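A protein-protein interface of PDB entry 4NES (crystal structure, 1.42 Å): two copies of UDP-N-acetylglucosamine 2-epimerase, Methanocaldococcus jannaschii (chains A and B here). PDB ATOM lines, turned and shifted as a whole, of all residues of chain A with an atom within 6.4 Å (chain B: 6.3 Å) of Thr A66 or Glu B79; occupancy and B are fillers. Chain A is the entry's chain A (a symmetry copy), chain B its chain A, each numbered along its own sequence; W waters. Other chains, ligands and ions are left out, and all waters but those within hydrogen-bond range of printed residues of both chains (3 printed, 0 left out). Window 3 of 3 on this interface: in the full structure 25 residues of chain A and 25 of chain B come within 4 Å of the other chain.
OE2 of Glu B79 touches N of His A67, at 3.6 Å.
Lys B108 touches His A67 (CB to CB, 3.6 Å).
Leu B75 touches Gly A68.
Gly A68 touches Ile B76 (O to N, 3.8 Å).
Glu A69 touches Ile B76 (O to CG1, 3.99 Å).
CD1 of Leu B75 touches CG2 of Thr A71 (3.7 Å).
Of chain B, only Glu B79 comes within 4 Å of Thr A66.
Of chain A, only Thr A66 (2.6 Å), His A67 (3.6 Å), Gly A68 (2.8 Å) and Glu A69 (3.0 Å) come within 4 Å of Glu B79.
Of the printed residues of chain B, Gly A68 touches Leu B75, Ile B76 and Glu B79.
Of the printed residues of chain A, Lys B108 touches His A67 (3.6 Å) and Asn A97 (2.8 Å).
Of the printed residues of chain A, Ile B76 touches Gly A68 (3.8 Å) and Glu A69 (3.99 Å).
Of the printed residues of chain B, His A67 touches Glu B79 (3.6 Å) and Lys B108 (3.6 Å).
Val B81 touches none of the printed residues of chain A.
Glu B77 touches none of the printed residues of chain A.
The nearest residue of chain B that does not touch Thr A66 is Leu B83 (4.6 Å).
The nearest residue of chain A that does not touch Glu B79 is Gln A70 (5.5 Å).
Of the 14 printed residues of chain B, 4 touch a printed residue of chain A.
Hydrophobic or aromatic side chains of chain B within 4 Å of the printed part of chain A: Leu B75 and Ile B76.
Of the 9 printed residues of chain A, 6 touch a printed residue of chain B.
Among the printed residues, 10 pairs touch across the chains.
Among the printed residues, no Asp or Glu carboxylate lies within 4 Å of a Lys or Arg side-chain nitrogen of the other chain.
The backbone NH (N) of Gly A68 lies within hydrogen-bond range of the side-chain carboxylate (OE2) of Glu B79, at 2.8 Å.
OG1 of Thr A66 is in hydrogen-bond range of OE1 of Glu B79, at 2.6 Å.
The side-chain carboxylate of Glu B79 is in hydrogen-bond range of the backbone NH of Glu A69 (3.0 Å).
NZ of Lys B108 lies within hydrogen-bond range of OD1 of Asn A97, 2.8 Å away.
No position is printed for both chains.
Of the 10 pairs that touch across the chains among the printed residues, none has its exchanged pair printed and touching as well.
Water W3 lies within hydrogen-bond range of NZ of Lys B108 and OG1 of Thr A71.
Water W2 lies within hydrogen-bond range of OE2 of Glu B79, O of Val B105 and N of Gly A68.
Water W1 bridges OE2 of Glu B79 (3.0 Å) and N of His A67 (3.0 Å).
ND2 of Asn A97 sits at hydrogen-bond distance from OE1 of Gln A70, at 2.9 Å.
The side-chain carboxylate of Glu A69 lies within hydrogen-bond range of the backbone NH of Thr A66.
ND2 of Asn A97 lies within hydrogen-bond range of ND1 of His A67 (3.0 Å).
The backbone carbonyl oxygen (O) of His A67 sits at hydrogen-bond distance from the side-chain hydroxyl (OG1) of Thr A71 (2.7 Å).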
ATOM      1  N   SER A  64     -15.852  35.980   0.357  1.00  0.00           N
ATOM      2  CA  SER A  64     -15.119  34.789   0.750  1.00  0.00           C
ATOM      3  C   SER A  64     -15.096  33.711  -0.320  1.00  0.00           C
ATOM      4  O   SER A  64     -15.945  33.672  -1.213  1.00  0.00           O
ATOM      5  CB  SER A  64     -15.706  34.221   2.038  1.00  0.00           C
ATOM      6  OG  SER A  64     -15.664  35.207   3.058  1.00  0.00           O
ATOM      7  N   GLY A  65     -14.115  32.826  -0.204  1.00  0.00           N
ATOM      8  CA  GLY A  65     -14.013  31.685  -1.089  1.00  0.00           C
ATOM      9  C   GLY A  65     -12.652  31.059  -0.940  1.00  0.00           C
ATOM     10  O   GLY A  65     -11.810  31.537  -0.173  1.00  0.00           O
ATOM     11  N   THR A  66     -12.426  29.981  -1.680  1.00  0.00           N
ATOM     12  CA  THR A  66     -11.109  29.374  -1.702  1.00  0.00           C
ATOM     13  C   THR A  66     -10.174  30.291  -2.487  1.00  0.00           C
ATOM     14  O   THR A  66     -10.628  31.217  -3.158  1.00  0.00           O
ATOM     15  CB  THR A  66     -11.155  27.964  -2.302  1.00  0.00           C
ATOM     16  OG1 THR A  66     -11.849  28.009  -3.549  1.00  0.00           O
ATOM     17  CG2 THR A  66     -11.901  27.018  -1.362  1.00  0.00           C
ATOM     18  N   HIS A  67      -8.874  30.045  -2.391  1.00  0.00           N
ATOM     19  CA  HIS A  67      -7.887  30.976  -2.934  1.00  0.00           C
ATOM     20  C   HIS A  67      -8.029  31.207  -4.427  1.00  0.00           C
ATOM     21  O   HIS A  67      -7.969  32.333  -4.890  1.00  0.00           O
ATOM     22  CB  HIS A  67      -6.463  30.498  -2.647  1.00  0.00           C
ATOM     23  CG  HIS A  67      -6.091  30.559  -1.203  1.00  0.00           C
ATOM     24  ND1 HIS A  67      -5.800  31.744  -0.562  1.00  0.00           N
ATOM     25  CD2 HIS A  67      -5.956  29.584  -0.277  1.00  0.00           C
ATOM     26  CE1 HIS A  67      -5.516  31.497   0.701  1.00  0.00           C
ATOM     27  NE2 HIS A  67      -5.600  30.192   0.904  1.00  0.00           N
ATOM     28  N   GLY A  68      -8.195  30.137  -5.196  1.00  0.00           N
ATOM     29  CA  GLY A  68      -8.288  30.284  -6.638  1.00  0.00           C
ATOM     30  C   GLY A  68      -9.565  30.987  -7.044  1.00  0.00           C
ATOM     31  O   GLY A  68      -9.552  31.875  -7.902  1.00  0.00           O
ATOM     32  N   GLU A  69     -10.670  30.614  -6.405  1.00  0.00           N
ATOM     33  CA  GLU A  69     -11.963  31.243  -6.654  1.00  0.00           C
ATOM     34  C   GLU A  69     -11.929  32.741  -6.333  1.00  0.00           C
ATOM     35  O   GLU A  69     -12.302  33.579  -7.155  1.00  0.00           O
ATOM     36  CB  GLU A  69     -13.042  30.539  -5.819  1.00  0.00           C
ATOM     37  CG  GLU A  69     -14.408  31.206  -5.852  1.00  0.00           C
ATOM     38  CD  GLU A  69     -15.324  30.749  -4.722  1.00  0.00           C
ATOM     39  OE1 GLU A  69     -14.862  30.015  -3.819  1.00  0.00           O
ATOM     40  OE2 GLU A  69     -16.512  31.134  -4.739  1.00  0.00           O
ATOM     41  N   GLN A  70     -11.455  33.074  -5.142  1.00  0.00           N
ATOM     42  CA  GLN A  70     -11.445  34.449  -4.670  1.00  0.00           C
ATOM     43  C   GLN A  70     -10.461  35.299  -5.471  1.00  0.00           C
ATOM     44  O   GLN A  70     -10.810  36.378  -5.954  1.00  0.00           O
ATOM     45  CB  GLN A  70     -11.073  34.445  -3.191  1.00  0.00           C
ATOM     46  CG  GLN A  70     -11.151  35.783  -2.503  1.00  0.00           C
ATOM     47  CD  GLN A  70     -10.664  35.686  -1.074  1.00  0.00           C
ATOM     48  OE1 GLN A  70      -9.486  35.432  -0.834  1.00  0.00           O
ATOM     49  NE2 GLN A  70     -11.571  35.862  -0.117  1.00  0.00           N
ATOM     50  N   THR A  71      -9.237  34.801  -5.639  1.00  0.00           N
ATOM     51  CA  THR A  71      -8.220  35.554  -6.371  1.00  0.00           C
ATOM     52  C   THR A  71      -8.613  35.687  -7.845  1.00  0.00           C
ATOM     53  O   THR A  71      -8.440  36.744  -8.439  1.00  0.00           O
ATOM     54  CB  THR A  71      -6.840  34.893  -6.248  1.00  0.00           C
ATOM     55  OG1 THR A  71      -6.542  34.668  -4.862  1.00  0.00           O
ATOM     56  CG2 THR A  71      -5.752  35.766  -6.860  1.00  0.00           C
ATOM     57  N   ASN A  97      -4.876  38.203  -0.269  1.00  0.00           N
ATOM     58  CA  ASN A  97      -5.187  37.865  -1.659  1.00  0.00           C
ATOM     59  C   ASN A  97      -5.548  39.100  -2.487  1.00  0.00           C
ATOM     60  O   ASN A  97      -5.250  39.157  -3.676  1.00  0.00           O
ATOM     61  CB  ASN A  97      -6.295  36.817  -1.751  1.00  0.00           C
ATOM     62  CG  ASN A  97      -5.819  35.432  -1.378  1.00  0.00           C
ATOM     63  OD1 ASN A  97      -4.622  35.189  -1.210  1.00  0.00           O
ATOM     64  ND2 ASN A  97      -6.761  34.501  -1.256  1.00  0.00           N
ATOM     65  N   MET B  74      -8.823  31.056 -15.376  1.00  0.00           N
ATOM     66  CA  MET B  74      -7.947  29.908 -15.172  1.00  0.00           C
ATOM     67  C   MET B  74      -7.788  29.547 -13.700  1.00  0.00           C
ATOM     68  O   MET B  74      -7.819  28.371 -13.356  1.00  0.00           O
ATOM     69  CB  MET B  74      -6.570  30.143 -15.800  1.00  0.00           C
ATOM     70  CG  MET B  74      -6.558  30.170 -17.306  1.00  0.00           C
ATOM     71  SD  MET B  74      -4.846  30.797 -18.004  1.00  0.00           S
ATOM     72  CE  MET B  74      -5.231  30.452 -19.876  1.00  0.00           C
ATOM     73  N   LEU B  75      -7.615  30.540 -12.826  1.00  0.00           N
ATOM     74  CA  LEU B  75      -7.500  30.253 -11.392  1.00  0.00           C
ATOM     75  C   LEU B  75      -8.759  29.567 -10.884  1.00  0.00           C
ATOM     76  O   LEU B  75      -8.685  28.583 -10.142  1.00  0.00           O
ATOM     77  CB  LEU B  75      -7.273  31.525 -10.566  1.00  0.00           C
ATOM     78  CG  LEU B  75      -5.993  32.324 -10.808  1.00  0.00           C
ATOM     79  CD1 LEU B  75      -5.901  33.500  -9.835  1.00  0.00           C
ATOM     80  CD2 LEU B  75      -4.768  31.440 -10.678  1.00  0.00           C
ATOM     81  N   ILE B  76      -9.919  30.088 -11.272  1.00  0.00           N
ATOM     82  CA  ILE B  76     -11.182  29.488 -10.848  1.00  0.00           C
ATOM     83  C   ILE B  76     -11.325  28.048 -11.333  1.00  0.00           C
ATOM     84  O   ILE B  76     -11.638  27.148 -10.547  1.00  0.00           O
ATOM     85  CB  ILE B  76     -12.386  30.323 -11.330  1.00  0.00           C
ATOM     86  CG1 ILE B  76     -12.354  31.703 -10.678  1.00  0.00           C
ATOM     87  CG2 ILE B  76     -13.696  29.622 -11.003  1.00  0.00           C
ATOM     88  CD1 ILE B  76     -13.126  32.745 -11.451  1.00  0.00           C
ATOM     89  N   GLU B  77     -11.084  27.826 -12.616  1.00  0.00           N
ATOM     90  CA  GLU B  77     -11.366  26.524 -13.206  1.00  0.00           C
ATOM     91  C   GLU B  77     -10.302  25.476 -12.908  1.00  0.00           C
ATOM     92  O   GLU B  77     -10.633  24.309 -12.699  1.00  0.00           O
ATOM     93  CB  GLU B  77     -11.584  26.646 -14.715  1.00  0.00           C
ATOM     94  CG  GLU B  77     -12.800  27.482 -15.082  1.00  0.00           C
ATOM     95  CD  GLU B  77     -14.086  26.943 -14.490  1.00  0.00           C
ATOM     96  OE1 GLU B  77     -14.300  25.717 -14.544  1.00  0.00           O
ATOM     97  OE2 GLU B  77     -14.891  27.751 -13.986  1.00  0.00           O
ATOM     98  N   ILE B  78      -9.038  25.883 -12.862  1.00  0.00           N
ATOM     99  CA  ILE B  78      -7.982  24.944 -12.505  1.00  0.00           C
ATOM    100  C   ILE B  78      -8.180  24.508 -11.060  1.00  0.00           C
ATOM    101  O   ILE B  78      -8.002  23.343 -10.730  1.00  0.00           O
ATOM    102  CB  ILE B  78      -6.571  25.548 -12.689  1.00  0.00           C
ATOM    103  CG1 ILE B  78      -6.255  25.750 -14.165  1.00  0.00           C
ATOM    104  CG2 ILE B  78      -5.497  24.657 -12.095  1.00  0.00           C
ATOM    105  CD1 ILE B  78      -4.941  26.485 -14.388  1.00  0.00           C
ATOM    106  N   GLU B  79      -8.575  25.428 -10.189  1.00  0.00           N
ATOM    107  CA  GLU B  79      -8.751  25.059  -8.793  1.00  0.00           C
ATOM    108  C   GLU B  79      -9.850  24.023  -8.603  1.00  0.00           C
ATOM    109  O   GLU B  79      -9.710  23.125  -7.778  1.00  0.00           O
ATOM    110  CB  GLU B  79      -9.026  26.280  -7.927  1.00  0.00           C
ATOM    111  CG  GLU B  79      -9.108  25.917  -6.455  1.00  0.00           C
ATOM    112  CD  GLU B  79      -9.333  27.099  -5.568  1.00  0.00           C
ATOM    113  OE1 GLU B  79     -10.396  27.734  -5.707  1.00  0.00           O
ATOM    114  OE2 GLU B  79      -8.446  27.383  -4.729  1.00  0.00           O
ATOM    115  N   LYS B  80     -10.935  24.135  -9.364  1.00  0.00           N
ATOM    116  CA  LYS B  80     -12.002  23.142  -9.284  1.00  0.00           C
ATOM    117  C   LYS B  80     -11.475  21.739  -9.582  1.00  0.00           C
ATOM    118  O   LYS B  80     -11.788  20.780  -8.864  1.00  0.00           O
ATOM    119  CB  LYS B  80     -13.129  23.485 -10.252  1.00  0.00           C
ATOM    120  CG  LYS B  80     -13.951  24.698  -9.851  1.00  0.00           C
ATOM    121  CD  LYS B  80     -14.973  25.023 -10.939  1.00  0.00           C
ATOM    122  CE  LYS B  80     -15.766  26.271 -10.613  1.00  0.00           C
ATOM    123  NZ  LYS B  80     -16.657  26.645 -11.751  1.00  0.00           N
ATOM    124  N   VAL B  81     -10.651  21.622 -10.620  1.00  0.00           N
ATOM    125  CA  VAL B  81     -10.062  20.339 -10.967  1.00  0.00           C
ATOM    126  C   VAL B  81      -9.092  19.840  -9.903  1.00  0.00           C
ATOM    127  O   VAL B  81      -9.161  18.677  -9.501  1.00  0.00           O
ATOM    128  CB  VAL B  81      -9.348  20.395 -12.318  1.00  0.00           C
ATOM    129  CG1 VAL B  81      -8.693  19.048 -12.606  1.00  0.00           C
ATOM    130  CG2 VAL B  81     -10.331  20.760 -13.422  1.00  0.00           C
ATOM    131  N   LEU B  82      -8.204  20.710  -9.427  1.00  0.00           N
ATOM    132  CA  LEU B  82      -7.196  20.272  -8.461  1.00  0.00           C
ATOM    133  C   LEU B  82      -7.792  19.905  -7.102  1.00  0.00           C
ATOM    134  O   LEU B  82      -7.272  19.018  -6.419  1.00  0.00           O
ATOM    135  CB  LEU B  82      -6.065  21.297  -8.312  1.00  0.00           C
ATOM    136  CG  LEU B  82      -5.236  21.547  -9.577  1.00  0.00           C
ATOM    137  CD1 LEU B  82      -4.093  22.500  -9.276  1.00  0.00           C
ATOM    138  CD2 LEU B  82      -4.712  20.245 -10.185  1.00  0.00           C
ATOM    139  N   LEU B  83      -8.875  20.575  -6.711  1.00  0.00           N
ATOM    140  CA  LEU B  83      -9.597  20.206  -5.491  1.00  0.00           C
ATOM    141  C   LEU B  83     -10.231  18.819  -5.589  1.00  0.00           C
ATOM    142  O   LEU B  83     -10.364  18.119  -4.582  1.00  0.00           O
ATOM    143  CB  LEU B  83     -10.673  21.243  -5.169  1.00  0.00           C
ATOM    144  CG  LEU B  83     -10.158  22.543  -4.552  1.00  0.00           C
ATOM    145  CD1 LEU B  83     -11.271  23.575  -4.469  1.00  0.00           C
ATOM    146  CD2 LEU B  83      -9.563  22.290  -3.175  1.00  0.00           C
ATOM    147  N   LYS B  84     -10.631  18.433  -6.797  1.00  0.00           N
ATOM    148  CA  LYS B  84     -11.234  17.130  -7.020  1.00  0.00           C
ATOM    149  C   LYS B  84     -10.183  16.041  -7.139  1.00  0.00           C
ATOM    150  O   LYS B  84     -10.284  14.998  -6.486  1.00  0.00           O
ATOM    151  CB  LYS B  84     -12.088  17.147  -8.280  1.00  0.00           C
ATOM    152  CG  LYS B  84     -12.566  15.769  -8.681  1.00  0.00           C
ATOM    153  CD  LYS B  84     -13.313  15.811  -9.998  1.00  0.00           C
ATOM    154  CE  LYS B  84     -13.880  14.451 -10.339  1.00  0.00           C
ATOM    155  NZ  LYS B  84     -14.710  14.504 -11.568  1.00  0.00           N
ATOM    156  N   VAL B 105      -2.483  28.412  -8.471  1.00  0.00           N
ATOM    157  CA  VAL B 105      -3.509  27.579  -7.859  1.00  0.00           C
ATOM    158  C   VAL B 105      -2.859  26.507  -6.993  1.00  0.00           C
ATOM    159  O   VAL B 105      -3.228  26.324  -5.834  1.00  0.00           O
ATOM    160  CB  VAL B 105      -4.421  26.894  -8.906  1.00  0.00           C
ATOM    161  CG1 VAL B 105      -5.312  25.864  -8.227  1.00  0.00           C
ATOM    162  CG2 VAL B 105      -5.269  27.915  -9.649  1.00  0.00           C
ATOM    163  N   LYS B 108      -1.237  27.677  -3.545  1.00  0.00           N
ATOM    164  CA  LYS B 108      -2.165  27.961  -2.454  1.00  0.00           C
ATOM    165  C   LYS B 108      -2.839  26.696  -1.924  1.00  0.00           C
ATOM    166  O   LYS B 108      -3.311  26.670  -0.795  1.00  0.00           O
ATOM    167  CB  LYS B 108      -3.224  28.984  -2.876  1.00  0.00           C
ATOM    168  CG  LYS B 108      -2.674  30.387  -3.169  1.00  0.00           C
ATOM    169  CD  LYS B 108      -2.190  31.071  -1.884  1.00  0.00           C
ATOM    170  CE  LYS B 108      -1.691  32.495  -2.148  1.00  0.00           C
ATOM    171  NZ  LYS B 108      -2.803  33.445  -2.481  1.00  0.00           N
ATOM    172  N   LEU B 109      -2.879  25.643  -2.742  1.00  0.00           N
ATOM    173  CA  LEU B 109      -3.416  24.359  -2.310  1.00  0.00           C
ATOM    174  C   LEU B 109      -2.345  23.492  -1.658  1.00  0.00           C
ATOM    175  O   LEU B 109      -2.623  22.363  -1.247  1.00  0.00           O
ATOM    176  CB  LEU B 109      -4.025  23.604  -3.490  1.00  0.00           C
ATOM    177  CG  LEU B 109      -5.319  24.160  -4.097  1.00  0.00           C
ATOM    178  CD1 LEU B 109      -5.789  23.272  -5.250  1.00  0.00           C
ATOM    179  CD2 LEU B 109      -6.415  24.303  -3.046  1.00  0.00           C
HETATM  180  O   HOH W   1      -7.823  27.331  -1.845  1.00  0.00           O
HETATM  181  O   HOH W   2      -5.630  27.919  -5.156  1.00  0.00           O
HETATM  182  O   HOH W   3      -4.174  33.044  -4.814  1.00  0.00           O
